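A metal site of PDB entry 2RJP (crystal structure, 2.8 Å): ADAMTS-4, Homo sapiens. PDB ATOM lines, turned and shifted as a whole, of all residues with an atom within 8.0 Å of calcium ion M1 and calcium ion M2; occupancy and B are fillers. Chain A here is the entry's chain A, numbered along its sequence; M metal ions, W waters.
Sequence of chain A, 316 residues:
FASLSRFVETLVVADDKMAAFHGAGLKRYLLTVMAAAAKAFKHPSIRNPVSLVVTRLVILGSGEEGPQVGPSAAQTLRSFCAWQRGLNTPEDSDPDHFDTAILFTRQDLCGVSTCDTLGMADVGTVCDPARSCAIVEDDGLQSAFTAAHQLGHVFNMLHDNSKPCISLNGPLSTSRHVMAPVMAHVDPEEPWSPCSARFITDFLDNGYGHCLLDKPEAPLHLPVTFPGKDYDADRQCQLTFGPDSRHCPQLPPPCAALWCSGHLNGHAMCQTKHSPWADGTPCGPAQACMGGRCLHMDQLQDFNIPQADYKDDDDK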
ATOM      1  N   ARG A   6      -1.411 -18.523  -3.219  1.00  0.00           N
ATOM      2  CA  ARG A   6      -2.302 -17.670  -3.981  1.00  0.00           C
ATOM      3  C   ARG A   6      -1.737 -17.358  -5.354  1.00  0.00           C
ATOM      4  O   ARG A   6      -0.526 -17.211  -5.516  1.00  0.00           O
ATOM      5  CB  ARG A   6      -2.601 -16.393  -3.195  1.00  0.00           C
ATOM      6  CG  ARG A   6      -3.685 -16.619  -2.123  1.00  0.00           C
ATOM      7  CD  ARG A   6      -3.527 -15.728  -0.894  1.00  0.00           C
ATOM      8  NE  ARG A   6      -4.227 -16.282   0.265  1.00  0.00           N
ATOM      9  CZ  ARG A   6      -5.537 -16.142   0.496  1.00  0.00           C
ATOM     10  NH1 ARG A   6      -6.309 -15.464  -0.332  1.00  0.00           N
ATOM     11  NH2 ARG A   6      -6.077 -16.694   1.573  1.00  0.00           N
ATOM     12  N   PHE A   7      -2.625 -17.274  -6.341  1.00  0.00           N
ATOM     13  CA  PHE A   7      -2.235 -17.021  -7.722  1.00  0.00           C
ATOM     14  C   PHE A   7      -2.983 -15.811  -8.262  1.00  0.00           C
ATOM     15  O   PHE A   7      -4.209 -15.757  -8.212  1.00  0.00           O
ATOM     16  CB  PHE A   7      -2.506 -18.266  -8.582  1.00  0.00           C
ATOM     17  CG  PHE A   7      -1.837 -19.496  -8.054  1.00  0.00           C
ATOM     18  CD1 PHE A   7      -2.497 -20.335  -7.148  1.00  0.00           C
ATOM     19  CD2 PHE A   7      -0.545 -19.820  -8.439  1.00  0.00           C
ATOM     20  CE1 PHE A   7      -1.881 -21.476  -6.642  1.00  0.00           C
ATOM     21  CE2 PHE A   7       0.087 -20.957  -7.932  1.00  0.00           C
ATOM     22  CZ  PHE A   7      -0.580 -21.790  -7.029  1.00  0.00           C
ATOM     23  N   VAL A   8      -2.229 -14.834  -8.758  1.00  0.00           N
ATOM     24  CA  VAL A   8      -2.824 -13.638  -9.355  1.00  0.00           C
ATOM     25  C   VAL A   8      -2.817 -13.770 -10.864  1.00  0.00           C
ATOM     26  O   VAL A   8      -1.800 -13.540 -11.520  1.00  0.00           O
ATOM     27  CB  VAL A   8      -2.123 -12.319  -8.944  1.00  0.00           C
ATOM     28  CG1 VAL A   8      -2.847 -11.111  -9.562  1.00  0.00           C
ATOM     29  CG2 VAL A   8      -2.055 -12.178  -7.443  1.00  0.00           C
ATOM     30  N   GLU A   9      -3.959 -14.171 -11.409  1.00  0.00           N
ATOM     31  CA  GLU A   9      -4.082 -14.386 -12.840  1.00  0.00           C
ATOM     32  C   GLU A   9      -4.215 -13.010 -13.483  1.00  0.00           C
ATOM     33  O   GLU A   9      -5.174 -12.275 -13.203  1.00  0.00           O
ATOM     34  CB  GLU A   9      -5.261 -15.315 -13.138  1.00  0.00           C
ATOM     35  CG  GLU A   9      -5.083 -16.715 -12.528  1.00  0.00           C
ATOM     36  CD  GLU A   9      -6.323 -17.596 -12.648  1.00  0.00           C
ATOM     37  OE1 GLU A   9      -7.311 -17.374 -11.911  1.00  0.00           O
ATOM     38  OE2 GLU A   9      -6.298 -18.560 -13.452  1.00  0.00           O
ATOM     39  N   THR A  10      -3.233 -12.665 -14.319  1.00  0.00           N
ATOM     40  CA  THR A  10      -3.038 -11.295 -14.772  1.00  0.00           C
ATOM     41  C   THR A  10      -3.224 -11.111 -16.252  1.00  0.00           C
ATOM     42  O   THR A  10      -2.762 -11.923 -17.054  1.00  0.00           O
ATOM     43  CB  THR A  10      -1.633 -10.795 -14.388  1.00  0.00           C
ATOM     44  OG1 THR A  10      -1.445 -10.953 -12.972  1.00  0.00           O
ATOM     45  CG2 THR A  10      -1.447  -9.324 -14.771  1.00  0.00           C
ATOM     46  N   THR A  55      -1.719 -14.755 -17.523  1.00  0.00           N
ATOM     47  CA  THR A  55      -2.579 -15.694 -18.219  1.00  0.00           C
ATOM     48  C   THR A  55      -3.019 -15.168 -19.583  1.00  0.00           C
ATOM     49  O   THR A  55      -3.306 -15.943 -20.505  1.00  0.00           O
ATOM     50  CB  THR A  55      -3.804 -16.139 -17.367  1.00  0.00           C
ATOM     51  OG1 THR A  55      -4.645 -15.013 -17.104  1.00  0.00           O
ATOM     52  CG2 THR A  55      -3.361 -16.749 -16.054  1.00  0.00           C
ATOM     53  N   THR A  89     -14.662 -12.495 -17.842  1.00  0.00           N
ATOM     54  CA  THR A  89     -15.715 -13.504 -17.958  1.00  0.00           C
ATOM     55  C   THR A  89     -16.425 -13.660 -16.613  1.00  0.00           C
ATOM     56  O   THR A  89     -15.815 -13.455 -15.565  1.00  0.00           O
ATOM     57  CB  THR A  89     -15.159 -14.893 -18.352  1.00  0.00           C
ATOM     58  OG1 THR A  89     -14.486 -15.474 -17.231  1.00  0.00           O
ATOM     59  CG2 THR A  89     -14.190 -14.792 -19.539  1.00  0.00           C
ATOM     60  N   GLU A  91     -17.356 -16.282 -14.572  1.00  0.00           N
ATOM     61  CA  GLU A  91     -16.754 -17.141 -13.544  1.00  0.00           C
ATOM     62  C   GLU A  91     -15.236 -17.319 -13.658  1.00  0.00           C
ATOM     63  O   GLU A  91     -14.653 -17.128 -14.733  1.00  0.00           O
ATOM     64  CB  GLU A  91     -17.452 -18.520 -13.506  1.00  0.00           C
ATOM     65  CG  GLU A  91     -18.702 -18.548 -12.615  1.00  0.00           C
ATOM     66  CD  GLU A  91     -19.649 -19.702 -12.923  1.00  0.00           C
ATOM     67  OE1 GLU A  91     -19.516 -20.314 -14.008  1.00  0.00           O
ATOM     68  OE2 GLU A  91     -20.536 -19.979 -12.092  1.00  0.00           O
ATOM     69  N   ASP A  92     -14.604 -17.689 -12.543  1.00  0.00           N
ATOM     70  CA  ASP A  92     -13.154 -17.917 -12.491  1.00  0.00           C
ATOM     71  C   ASP A  92     -12.800 -19.362 -12.846  1.00  0.00           C
ATOM     72  O   ASP A  92     -11.628 -19.764 -12.852  1.00  0.00           O
ATOM     73  CB  ASP A  92     -12.587 -17.542 -11.103  1.00  0.00           C
ATOM     74  CG  ASP A  92     -11.101 -17.199 -11.146  1.00  0.00           C
ATOM     75  OD1 ASP A  92     -10.473 -17.289 -12.234  1.00  0.00           O
ATOM     76  OD2 ASP A  92     -10.544 -16.828 -10.096  1.00  0.00           O
ATOM     77  N   SER A  93     -13.827 -20.151 -13.153  1.00  0.00           N
ATOM     78  CA  SER A  93     -13.649 -21.494 -13.688  1.00  0.00           C
ATOM     79  C   SER A  93     -13.088 -21.411 -15.122  1.00  0.00           C
ATOM     80  O   SER A  93     -12.270 -22.240 -15.521  1.00  0.00           O
ATOM     81  CB  SER A  93     -14.977 -22.242 -13.662  1.00  0.00           C
ATOM     82  OG  SER A  93     -14.964 -23.362 -14.524  1.00  0.00           O
ATOM     83  N   ASP A  94     -13.549 -20.405 -15.861  1.00  0.00           N
ATOM     84  CA  ASP A  94     -13.210 -20.243 -17.269  1.00  0.00           C
ATOM     85  C   ASP A  94     -11.758 -19.798 -17.445  1.00  0.00           C
ATOM     86  O   ASP A  94     -11.365 -18.743 -16.934  1.00  0.00           O
ATOM     87  CB  ASP A  94     -14.166 -19.246 -17.929  1.00  0.00           C
ATOM     88  CG  ASP A  94     -14.159 -19.331 -19.442  1.00  0.00           C
ATOM     89  OD1 ASP A  94     -13.126 -18.978 -20.053  1.00  0.00           O
ATOM     90  OD2 ASP A  94     -15.181 -19.746 -20.027  1.00  0.00           O
ATOM     91  N   PRO A  95     -10.938 -20.592 -18.169  1.00  0.00           N
ATOM     92  CA  PRO A  95      -9.509 -20.311 -18.388  1.00  0.00           C
ATOM     93  C   PRO A  95      -9.205 -18.920 -18.965  1.00  0.00           C
ATOM     94  O   PRO A  95      -8.042 -18.534 -19.045  1.00  0.00           O
ATOM     95  CB  PRO A  95      -9.085 -21.390 -19.399  1.00  0.00           C
ATOM     96  CG  PRO A  95     -10.365 -21.936 -19.954  1.00  0.00           C
ATOM     97  CD  PRO A  95     -11.353 -21.829 -18.851  1.00  0.00           C
ATOM     98  N   ASP A  96     -10.251 -18.190 -19.356  1.00  0.00           N
ATOM     99  CA  ASP A  96     -10.098 -16.832 -19.870  1.00  0.00           C
ATOM    100  C   ASP A  96     -10.328 -15.742 -18.822  1.00  0.00           C
ATOM    101  O   ASP A  96     -10.113 -14.562 -19.114  1.00  0.00           O
ATOM    102  CB  ASP A  96     -11.005 -16.616 -21.083  1.00  0.00           C
ATOM    103  CG  ASP A  96     -10.334 -16.981 -22.405  1.00  0.00           C
ATOM    104  OD1 ASP A  96      -9.101 -16.770 -22.521  1.00  0.00           O
ATOM    105  OD2 ASP A  96     -11.027 -17.451 -23.322  1.00  0.00           O
ATOM    106  N   HIS A  97     -10.738 -16.124 -17.609  1.00  0.00           N
ATOM    107  CA  HIS A  97     -10.928 -15.191 -16.502  1.00  0.00           C
ATOM    108  C   HIS A  97      -9.592 -14.710 -15.953  1.00  0.00           C
ATOM    109  O   HIS A  97      -8.641 -15.490 -15.877  1.00  0.00           O
ATOM    110  CB  HIS A  97     -11.741 -15.831 -15.372  1.00  0.00           C
ATOM    111  CG  HIS A  97     -12.144 -14.880 -14.289  1.00  0.00           C
ATOM    112  ND1 HIS A  97     -13.315 -14.161 -14.326  1.00  0.00           N
ATOM    113  CD2 HIS A  97     -11.520 -14.531 -13.136  1.00  0.00           C
ATOM    114  CE1 HIS A  97     -13.402 -13.411 -13.248  1.00  0.00           C
ATOM    115  NE2 HIS A  97     -12.333 -13.617 -12.508  1.00  0.00           N
ATOM    116  N   PHE A  98      -9.518 -13.437 -15.589  1.00  0.00           N
ATOM    117  CA  PHE A  98      -8.329 -12.860 -14.965  1.00  0.00           C
ATOM    118  C   PHE A  98      -8.686 -12.088 -13.698  1.00  0.00           C
ATOM    119  O   PHE A  98      -9.752 -11.486 -13.612  1.00  0.00           O
ATOM    120  CB  PHE A  98      -7.551 -11.962 -15.929  1.00  0.00           C
ATOM    121  CG  PHE A  98      -8.377 -10.857 -16.563  1.00  0.00           C
ATOM    122  CD1 PHE A  98      -8.543  -9.639 -15.922  1.00  0.00           C
ATOM    123  CD2 PHE A  98      -8.975 -11.044 -17.805  1.00  0.00           C
ATOM    124  CE1 PHE A  98      -9.300  -8.620 -16.496  1.00  0.00           C
ATOM    125  CE2 PHE A  98      -9.734 -10.036 -18.398  1.00  0.00           C
ATOM    126  CZ  PHE A  98      -9.895  -8.821 -17.741  1.00  0.00           C
ATOM    127  N   ASP A  99      -7.784 -12.111 -12.725  1.00  0.00           N
ATOM    128  CA  ASP A  99      -8.062 -11.493 -11.425  1.00  0.00           C
ATOM    129  C   ASP A  99      -7.561 -10.048 -11.306  1.00  0.00           C
ATOM    130  O   ASP A  99      -7.922  -9.346 -10.354  1.00  0.00           O
ATOM    131  CB  ASP A  99      -7.474 -12.346 -10.297  1.00  0.00           C
ATOM    132  CG  ASP A  99      -7.997 -13.778 -10.319  1.00  0.00           C
ATOM    133  OD1 ASP A  99      -9.233 -14.001 -10.185  1.00  0.00           O
ATOM    134  OD2 ASP A  99      -7.152 -14.693 -10.450  1.00  0.00           O
ATOM    135  N   THR A 100      -6.736  -9.615 -12.251  1.00  0.00           N
ATOM    136  CA  THR A 100      -6.132  -8.283 -12.193  1.00  0.00           C
ATOM    137  C   THR A 100      -5.737  -7.832 -13.594  1.00  0.00           C
ATOM    138  O   THR A 100      -5.394  -8.661 -14.436  1.00  0.00           O
ATOM    139  CB  THR A 100      -4.901  -8.258 -11.227  1.00  0.00           C
ATOM    140  OG1 THR A 100      -5.002  -7.151 -10.328  1.00  0.00           O
ATOM    141  CG2 THR A 100      -3.565  -8.197 -11.975  1.00  0.00           C
ATOM    142  N   CYS A 127      -9.994  -8.659  -5.824  1.00  0.00           N
ATOM    143  CA  CYS A 127     -11.056  -9.592  -6.173  1.00  0.00           C
ATOM    144  C   CYS A 127     -12.358  -8.918  -6.641  1.00  0.00           C
ATOM    145  O   CYS A 127     -13.420  -9.562  -6.732  1.00  0.00           O
ATOM    146  CB  CYS A 127     -11.306 -10.563  -5.027  1.00  0.00           C
ATOM    147  SG  CYS A 127      -9.977 -11.765  -4.833  1.00  0.00           S
ATOM    148  N   GLY A 209      -9.098 -11.921  -0.736  1.00  0.00           N
ATOM    149  CA  GLY A 209      -8.331 -12.571  -1.797  1.00  0.00           C
ATOM    150  C   GLY A 209      -8.920 -13.892  -2.274  1.00  0.00           C
ATOM    151  O   GLY A 209      -8.201 -14.725  -2.824  1.00  0.00           O
ATOM    152  N   HIS A 210     -10.221 -14.070  -2.072  1.00  0.00           N
ATOM    153  CA  HIS A 210     -10.902 -15.330  -2.400  1.00  0.00           C
ATOM    154  C   HIS A 210     -10.687 -15.758  -3.852  1.00  0.00           C
ATOM    155  O   HIS A 210     -10.553 -16.952  -4.136  1.00  0.00           O
ATOM    156  CB  HIS A 210     -12.400 -15.241  -2.077  1.00  0.00           C
ATOM    157  CG  HIS A 210     -13.129 -14.193  -2.868  1.00  0.00           C
ATOM    158  ND1 HIS A 210     -13.935 -14.295  -3.952  1.00  0.00           N
ATOM    159  CD2 HIS A 210     -13.078 -12.852  -2.553  1.00  0.00           C
ATOM    160  CE1 HIS A 210     -14.352 -13.023  -4.267  1.00  0.00           C
ATOM    161  NE2 HIS A 210     -13.824 -12.173  -3.414  1.00  0.00           N
ATOM    162  N   CYS A 211     -10.645 -14.779  -4.747  1.00  0.00           N
ATOM    163  CA  CYS A 211     -10.485 -15.017  -6.173  1.00  0.00           C
ATOM    164  C   CYS A 211      -9.090 -15.508  -6.591  1.00  0.00           C
ATOM    165  O   CYS A 211      -8.833 -15.691  -7.776  1.00  0.00           O
ATOM    166  CB  CYS A 211     -10.827 -13.748  -6.963  1.00  0.00           C
ATOM    167  SG  CYS A 211      -9.615 -12.409  -6.734  1.00  0.00           S
ATOM    168  N   LEU A 212      -8.210 -15.706  -5.613  1.00  0.00           N
ATOM    169  CA  LEU A 212      -6.810 -16.007  -5.909  1.00  0.00           C
ATOM    170  C   LEU A 212      -6.423 -17.434  -5.559  1.00  0.00           C
ATOM    171  O   LEU A 212      -5.245 -17.797  -5.648  1.00  0.00           O
ATOM    172  CB  LEU A 212      -5.875 -15.041  -5.174  1.00  0.00           C
ATOM    173  CG  LEU A 212      -6.014 -13.527  -5.345  1.00  0.00           C
ATOM    174  CD1 LEU A 212      -5.105 -12.840  -4.366  1.00  0.00           C
ATOM    175  CD2 LEU A 212      -5.705 -13.084  -6.784  1.00  0.00           C
ATOM    176  N   LEU A 213      -7.406 -18.235  -5.181  1.00  0.00           N
ATOM    177  CA  LEU A 213      -7.136 -19.565  -4.643  1.00  0.00           C
ATOM    178  C   LEU A 213      -6.939 -20.664  -5.693  1.00  0.00           C
ATOM    179  O   LEU A 213      -6.216 -21.627  -5.446  1.00  0.00           O
ATOM    180  CB  LEU A 213      -8.213 -19.972  -3.627  1.00  0.00           C
ATOM    181  CG  LEU A 213      -8.199 -19.206  -2.297  1.00  0.00           C
ATOM    182  CD1 LEU A 213      -9.514 -19.379  -1.562  1.00  0.00           C
ATOM    183  CD2 LEU A 213      -7.021 -19.632  -1.415  1.00  0.00           C
ATOM    184  N   ASP A 214      -7.571 -20.515  -6.862  1.00  0.00           N
ATOM    185  CA  ASP A 214      -7.422 -21.478  -7.959  1.00  0.00           C
ATOM    186  C   ASP A 214      -6.083 -21.346  -8.710  1.00  0.00           C
ATOM    187  O   ASP A 214      -5.531 -20.246  -8.814  1.00  0.00           O
ATOM    188  CB  ASP A 214      -8.583 -21.343  -8.957  1.00  0.00           C
ATOM    189  CG  ASP A 214      -8.585 -19.994  -9.665  1.00  0.00           C
ATOM    190  OD1 ASP A 214      -8.852 -18.974  -8.993  1.00  0.00           O
ATOM    191  OD2 ASP A 214      -8.299 -19.954 -10.880  1.00  0.00           O
ATOM    192  N   LYS A 215      -5.597 -22.463  -9.234  1.00  0.00           N
ATOM    193  CA  LYS A 215      -4.350 -22.469  -9.999  1.00  0.00           C
ATOM    194  C   LYS A 215      -4.636 -22.250 -11.494  1.00  0.00           C
ATOM    195  O   LYS A 215      -5.551 -22.854 -12.054  1.00  0.00           O
ATOM    196  CB  LYS A 215      -3.576 -23.777  -9.776  1.00  0.00           C
ATOM    197  CG  LYS A 215      -2.087 -23.648 -10.067  1.00  0.00           C
ATOM    198  CD  LYS A 215      -1.326 -24.966  -9.990  1.00  0.00           C
ATOM    199  CE  LYS A 215       0.138 -24.768 -10.397  1.00  0.00           C
ATOM    200  NZ  LYS A 215       0.829 -26.073 -10.641  1.00  0.00           N
ATOM    201  N   PRO A 216      -3.840 -21.370 -12.151  1.00  0.00           N
ATOM    202  CA  PRO A 216      -4.106 -20.983 -13.539  1.00  0.00           C
ATOM    203  C   PRO A 216      -4.023 -22.137 -14.538  1.00  0.00           C
ATOM    204  O   PRO A 216      -3.154 -23.017 -14.411  1.00  0.00           O
ATOM    205  CB  PRO A 216      -3.028 -19.942 -13.825  1.00  0.00           C
ATOM    206  CG  PRO A 216      -1.920 -20.283 -12.885  1.00  0.00           C
ATOM    207  CD  PRO A 216      -2.631 -20.712 -11.633  1.00  0.00           C
ATOM    208  N   GLU A 217      -4.901 -22.110 -15.531  1.00  0.00           N
ATOM    209  CA  GLU A 217      -4.994 -23.138 -16.570  1.00  0.00           C
ATOM    210  C   GLU A 217      -3.670 -23.356 -17.316  1.00  0.00           C
ATOM    211  O   GLU A 217      -3.102 -24.452 -17.283  1.00  0.00           O
ATOM    212  CB  GLU A 217      -6.109 -22.789 -17.550  1.00  0.00           C
ATOM    213  CG  GLU A 217      -6.255 -23.731 -18.742  1.00  0.00           C
ATOM    214  CD  GLU A 217      -7.207 -24.872 -18.480  1.00  0.00           C
ATOM    215  OE1 GLU A 217      -7.109 -25.515 -17.402  1.00  0.00           O
ATOM    216  OE2 GLU A 217      -8.073 -25.125 -19.350  1.00  0.00           O
HETATM  217 CA    CA M   1      -9.044 -19.062 -13.287  1.00  0.00          CA
HETATM  218 CA    CA M   2      -8.184 -16.815  -9.783  1.00  0.00          CA
HETATM  219  O   HOH W   1      -7.718 -21.074 -13.316  1.00  0.00           O
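Calcium ion M1 is bound by water W1 (2.4 Å), OD1 of Asp 92 (2.5 Å), OD2 of Asp 214 (2.7 Å), O of Asp 92 (2.7 Å), OE1 of Glu 9 (2.8 Å) and OE2 of Glu 9 (2.8 Å).
The side-chain carboxylate (OE1) of Glu 9 is bound to calcium ion M2 (2.4 Å). The side-chain carboxylate (OD2) of Asp 92 is bound to calcium ion M2. The backbone carbonyl oxygen (O) of Cys 211 is bound to calcium ion M2, 2.4 Å away. OD1 of Asp 214 binds calcium ion M2, 2.4 Å away. The side-chain carboxylate (OD2) of Asp 99 is bound to calcium ion M2. Calcium ion M2 has five donor atoms within binding distance. Slightly farther from calcium ion M2 lies the side-chain carboxylate (OD1) of Asp 99 (3.0 Å).
Within 4 Å of calcium ion M1: Glu 9, Asp 92 and Asp 214. The nearest printed residue that does not touch calcium ion M1 is Asp 94 (4.3 Å).
Of the 27 residues printed, 5 come within 4 Å of calcium ion M2. The nearest printed residue that does not touch calcium ion M2 is Leu 212 (4.2 Å).
The backbone NH of Thr 100 is in hydrogen-bond range of the backbone carbonyl oxygen of Glu 9, 3.2 Å away. SG of Cys 127 forms a disulfide with SG of Cys 211, at 2.0 Å.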
